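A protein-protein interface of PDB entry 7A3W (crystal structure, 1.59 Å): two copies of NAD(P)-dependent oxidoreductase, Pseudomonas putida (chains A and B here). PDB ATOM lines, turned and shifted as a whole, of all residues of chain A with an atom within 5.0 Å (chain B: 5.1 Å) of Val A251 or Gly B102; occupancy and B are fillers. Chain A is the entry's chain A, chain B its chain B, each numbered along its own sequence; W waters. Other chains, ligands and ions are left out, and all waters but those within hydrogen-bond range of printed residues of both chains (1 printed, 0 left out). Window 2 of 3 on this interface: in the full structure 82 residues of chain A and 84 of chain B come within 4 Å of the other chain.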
ATOM      1  N   ALA A 247      -1.792 -22.248 -24.128  1.00  0.00           N
ATOM      2  CA  ALA A 247      -2.879 -23.127 -24.603  1.00  0.00           C
ATOM      3  C   ALA A 247      -3.647 -23.653 -23.391  1.00  0.00           C
ATOM      4  O   ALA A 247      -4.882 -23.665 -23.441  1.00  0.00           O
ATOM      5  CB  ALA A 247      -2.343 -24.236 -25.452  1.00  0.00           C
ATOM      6  N   GLY A 248      -2.941 -24.043 -22.330  1.00  0.00           N
ATOM      7  CA  GLY A 248      -3.579 -24.522 -21.090  1.00  0.00           C
ATOM      8  C   GLY A 248      -4.400 -23.430 -20.415  1.00  0.00           C
ATOM      9  O   GLY A 248      -5.540 -23.694 -20.010  1.00  0.00           O
ATOM     10  N   GLN A 249      -3.826 -22.242 -20.243  1.00  0.00           N
ATOM     11  CA  GLN A 249      -4.495 -21.176 -19.460  1.00  0.00           C
ATOM     12  C   GLN A 249      -5.637 -20.583 -20.284  1.00  0.00           C
ATOM     13  O   GLN A 249      -6.512 -19.996 -19.657  1.00  0.00           O
ATOM     14  CB  GLN A 249      -3.532 -20.104 -18.948  1.00  0.00           C
ATOM     15  CG  GLN A 249      -3.920 -19.590 -17.572  1.00  0.00           C
ATOM     16  CD  GLN A 249      -3.649 -20.584 -16.455  1.00  0.00           C
ATOM     17  OE1 GLN A 249      -3.125 -21.670 -16.667  1.00  0.00           O
ATOM     18  NE2 GLN A 249      -4.015 -20.217 -15.235  1.00  0.00           N
ATOM     19  N   GLU A 250      -5.671 -20.779 -21.602  1.00  0.00           N
ATOM     20  CA  GLU A 250      -6.843 -20.338 -22.396  1.00  0.00           C
ATOM     21  C   GLU A 250      -8.040 -21.236 -22.057  1.00  0.00           C
ATOM     22  O   GLU A 250      -9.171 -20.761 -22.140  1.00  0.00           O
ATOM     23  CB  GLU A 250      -6.536 -20.327 -23.893  1.00  0.00           C
ATOM     24  CG  GLU A 250      -5.694 -19.135 -24.282  1.00  0.00           C
ATOM     25  CD  GLU A 250      -5.193 -19.145 -25.717  1.00  0.00           C
ATOM     26  OE1 GLU A 250      -5.116 -20.244 -26.321  1.00  0.00           O
ATOM     27  OE2 GLU A 250      -4.852 -18.062 -26.211  1.00  0.00           O
ATOM     28  N   VAL A 251      -7.798 -22.470 -21.633  1.00  0.00           N
ATOM     29  CA  VAL A 251      -8.867 -23.389 -21.145  1.00  0.00           C
ATOM     30  C   VAL A 251      -9.337 -22.897 -19.771  1.00  0.00           C
ATOM     31  O   VAL A 251     -10.548 -22.805 -19.543  1.00  0.00           O
ATOM     32  CB  VAL A 251      -8.369 -24.848 -21.110  1.00  0.00           C
ATOM     33  CG1 VAL A 251      -9.455 -25.797 -20.610  1.00  0.00           C
ATOM     34  CG2 VAL A 251      -7.880 -25.272 -22.486  1.00  0.00           C
ATOM     35  N   VAL A 252      -8.402 -22.521 -18.900  1.00  0.00           N
ATOM     36  CA  VAL A 252      -8.742 -21.935 -17.565  1.00  0.00           C
ATOM     37  C   VAL A 252      -9.600 -20.683 -17.802  1.00  0.00           C
ATOM     38  O   VAL A 252     -10.669 -20.551 -17.189  1.00  0.00           O
ATOM     39  CB  VAL A 252      -7.467 -21.648 -16.756  1.00  0.00           C
ATOM     40  CG1 VAL A 252      -7.785 -20.926 -15.466  1.00  0.00           C
ATOM     41  CG2 VAL A 252      -6.671 -22.933 -16.476  1.00  0.00           C
ATOM     42  N   LEU A 253      -9.186 -19.818 -18.723  1.00  0.00           N
ATOM     43  CA  LEU A 253      -9.912 -18.554 -18.995  1.00  0.00           C
ATOM     44  C   LEU A 253     -11.330 -18.889 -19.440  1.00  0.00           C
ATOM     45  O   LEU A 253     -12.274 -18.236 -18.985  1.00  0.00           O
ATOM     46  CB  LEU A 253      -9.174 -17.757 -20.063  1.00  0.00           C
ATOM     47  CG  LEU A 253      -9.883 -16.472 -20.496  1.00  0.00           C
ATOM     48  CD1 LEU A 253     -10.169 -15.565 -19.295  1.00  0.00           C
ATOM     49  CD2 LEU A 253      -9.046 -15.754 -21.545  1.00  0.00           C
ATOM     50  N   ASP A 254     -11.459 -19.816 -20.381  1.00  0.00           N
ATOM     51  CA  ASP A 254     -12.760 -20.251 -20.939  1.00  0.00           C
ATOM     52  C   ASP A 254     -13.675 -20.680 -19.781  1.00  0.00           C
ATOM     53  O   ASP A 254     -14.843 -20.312 -19.781  1.00  0.00           O
ATOM     54  CB  ASP A 254     -12.561 -21.388 -21.950  1.00  0.00           C
ATOM     55  CG  ASP A 254     -13.866 -22.026 -22.394  1.00  0.00           C
ATOM     56  OD1 ASP A 254     -14.604 -21.365 -23.160  1.00  0.00           O
ATOM     57  OD2 ASP A 254     -14.164 -23.138 -21.915  1.00  0.00           O
ATOM     58  N   ALA A 255     -13.181 -21.493 -18.855  1.00  0.00           N
ATOM     59  CA  ALA A 255     -13.957 -21.974 -17.691  1.00  0.00           C
ATOM     60  C   ALA A 255     -14.435 -20.786 -16.855  1.00  0.00           C
ATOM     61  O   ALA A 255     -15.621 -20.793 -16.441  1.00  0.00           O
ATOM     62  CB  ALA A 255     -13.132 -22.927 -16.872  1.00  0.00           C
ATOM     63  N   LYS B  75      -7.635 -32.178 -24.879  1.00  0.00           N
ATOM     64  CA  LYS B  75      -8.667 -33.233 -24.989  1.00  0.00           C
ATOM     65  C   LYS B  75      -9.266 -33.254 -26.397  1.00  0.00           C
ATOM     66  O   LYS B  75      -9.567 -34.337 -26.878  1.00  0.00           O
ATOM     67  CB  LYS B  75      -9.703 -33.031 -23.888  1.00  0.00           C
ATOM     68  CG  LYS B  75      -9.152 -33.245 -22.480  1.00  0.00           C
ATOM     69  CD  LYS B  75     -10.224 -33.251 -21.406  1.00  0.00           C
ATOM     70  CE  LYS B  75      -9.737 -33.033 -19.991  1.00  0.00           C
ATOM     71  NZ  LYS B  75      -8.841 -34.130 -19.521  1.00  0.00           N
ATOM     72  N   SER B 100      -4.707 -34.943 -20.453  1.00  0.00           N
ATOM     73  CA  SER B 100      -4.615 -33.760 -21.343  1.00  0.00           C
ATOM     74  C   SER B 100      -5.544 -32.661 -20.808  1.00  0.00           C
ATOM     75  O   SER B 100      -6.630 -32.979 -20.326  1.00  0.00           O
ATOM     76  CB  SER B 100      -4.922 -34.154 -22.764  1.00  0.00           C
ATOM     77  OG  SER B 100      -5.612 -33.120 -23.448  1.00  0.00           O
ATOM     78  N   THR B 101      -5.095 -31.410 -20.844  1.00  0.00           N
ATOM     79  CA  THR B 101      -5.903 -30.219 -20.497  1.00  0.00           C
ATOM     80  C   THR B 101      -7.047 -30.072 -21.498  1.00  0.00           C
ATOM     81  O   THR B 101      -6.823 -30.263 -22.689  1.00  0.00           O
ATOM     82  CB  THR B 101      -5.057 -28.945 -20.497  1.00  0.00           C
ATOM     83  OG1 THR B 101      -4.035 -29.108 -19.509  1.00  0.00           O
ATOM     84  CG2 THR B 101      -5.883 -27.708 -20.216  1.00  0.00           C
ATOM     85  N   GLY B 102      -8.246 -29.763 -21.001  1.00  0.00           N
ATOM     86  CA  GLY B 102      -9.442 -29.654 -21.852  1.00  0.00           C
ATOM     87  C   GLY B 102     -10.635 -29.205 -21.067  1.00  0.00           C
ATOM     88  O   GLY B 102     -10.545 -29.078 -19.850  1.00  0.00           O
ATOM     89  N   THR B 103     -11.735 -28.904 -21.760  1.00  0.00           N
ATOM     90  CA  THR B 103     -12.969 -28.351 -21.156  1.00  0.00           C
ATOM     91  C   THR B 103     -13.858 -29.492 -20.655  1.00  0.00           C
ATOM     92  O   THR B 103     -13.633 -30.655 -21.049  1.00  0.00           O
ATOM     93  CB  THR B 103     -13.743 -27.499 -22.164  1.00  0.00           C
ATOM     94  OG1 THR B 103     -14.843 -26.894 -21.491  1.00  0.00           O
ATOM     95  CG2 THR B 103     -14.308 -28.317 -23.297  1.00  0.00           C
ATOM     96  N   VAL B 104     -14.840 -29.175 -19.810  1.00  0.00           N
ATOM     97  CA  VAL B 104     -15.800 -30.190 -19.276  1.00  0.00           C
ATOM     98  C   VAL B 104     -16.615 -30.759 -20.446  1.00  0.00           C
ATOM     99  O   VAL B 104     -16.922 -31.959 -20.401  1.00  0.00           O
ATOM    100  CB  VAL B 104     -16.698 -29.613 -18.163  1.00  0.00           C
ATOM    101  CG1 VAL B 104     -16.772 -28.106 -18.216  1.00  0.00           C
ATOM    102  CG2 VAL B 104     -18.090 -30.225 -18.185  1.00  0.00           C
ATOM    103  N   ASP B 106     -15.495 -31.288 -23.535  1.00  0.00           N
ATOM    104  CA  ASP B 106     -14.587 -32.301 -24.122  1.00  0.00           C
ATOM    105  C   ASP B 106     -14.700 -33.591 -23.312  1.00  0.00           C
ATOM    106  O   ASP B 106     -14.784 -34.662 -23.919  1.00  0.00           O
ATOM    107  CB  ASP B 106     -13.110 -31.896 -24.093  1.00  0.00           C
ATOM    108  CG  ASP B 106     -12.721 -30.729 -24.981  1.00  0.00           C
ATOM    109  OD1 ASP B 106     -13.300 -30.598 -26.046  1.00  0.00           O
ATOM    110  OD2 ASP B 106     -11.807 -29.968 -24.573  1.00  0.00           O
ATOM    111  N   THR B 174     -11.849 -31.745 -14.011  1.00  0.00           N
ATOM    112  CA  THR B 174     -11.515 -30.563 -14.854  1.00  0.00           C
ATOM    113  C   THR B 174     -11.739 -29.244 -14.105  1.00  0.00           C
ATOM    114  O   THR B 174     -10.860 -28.385 -14.125  1.00  0.00           O
ATOM    115  CB  THR B 174     -12.218 -30.630 -16.216  1.00  0.00           C
ATOM    116  OG1 THR B 174     -11.432 -31.552 -16.963  1.00  0.00           O
ATOM    117  CG2 THR B 174     -12.255 -29.307 -16.949  1.00  0.00           C
ATOM    118  N   LEU B 178      -8.607 -26.858 -13.253  1.00  0.00           N
ATOM    119  CA  LEU B 178      -8.466 -25.518 -13.850  1.00  0.00           C
ATOM    120  C   LEU B 178      -8.445 -24.431 -12.758  1.00  0.00           C
ATOM    121  O   LEU B 178      -7.659 -23.449 -12.898  1.00  0.00           O
ATOM    122  CB  LEU B 178      -9.591 -25.317 -14.856  1.00  0.00           C
ATOM    123  CG  LEU B 178      -9.605 -26.230 -16.087  1.00  0.00           C
ATOM    124  CD1 LEU B 178     -10.831 -25.904 -16.941  1.00  0.00           C
ATOM    125  CD2 LEU B 178      -8.349 -26.108 -16.926  1.00  0.00           C
HETATM  126  O   HOH W   1     -12.893 -24.554 -20.207  1.00  0.00           O
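N of Thr B103 lies within hydrogen-bond range of OD2 of Asp B106, at 3.0 Å. The backbone carbonyl oxygen (O) of Thr B101 sits at hydrogen-bond distance from the backbone NH (N) of Lys B75, 3.0 Å away.
Val A251 touches Thr B101. O of Gly B102 touches CG1 of Val A251, 3.5 Å away. Leu B178 touches Val A251. Val A252 touches Leu B178. OD2 of Asp A254 touches OG1 of Thr B103, at 3.8 Å. CB of Ala A255 touches CD1 of Leu B178 (3.8 Å).
Gly B102 touches just one residue of chain A: Val A251 (3.5 Å). Of the printed residues of chain A, Leu B178 touches Val A251, Val A252 and Ala A255. Of the printed residues of chain B, Val A252 touches Leu B178 (3.6 Å). Of the printed residues of chain B, Ala A255 touches Leu B178 (3.8 Å). Printed residues of chain A within 4 Å of Thr B103: Asp A254. Printed residues of chain A within 4 Å of Thr B101: Val A251. Ser B100 touches none of the printed residues of chain A. The nearest printed residue of chain A that does not touch Gly B102 is Gly A248 (6.7 Å). The nearest printed residue of chain B that does not touch Asp A254 is Val B104 (6.4 Å).
Printed residues of chain B that touch a printed residue of chain A: Thr B101, Gly B102, Thr B103 and Leu B178. Hydrophobic or aromatic side chains of chain B within 4 Å of the printed part of chain A: Leu B178. Along chain A the printed residues that touch a printed residue of chain B span positions 251 to 255. Among the printed residues, no Asp or Glu carboxylate lies within 4 Å of a Lys or Arg side-chain nitrogen of the other chain.
No position is printed for both chains. Of the 6 pairs that touch across the chains among the printed residues, none has its exchanged pair printed and touching as well.
Water W1 lies within hydrogen-bond range of OD2 of Asp A254, O of Val A251, OG1 of Thr B103 and N of Ala A255.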
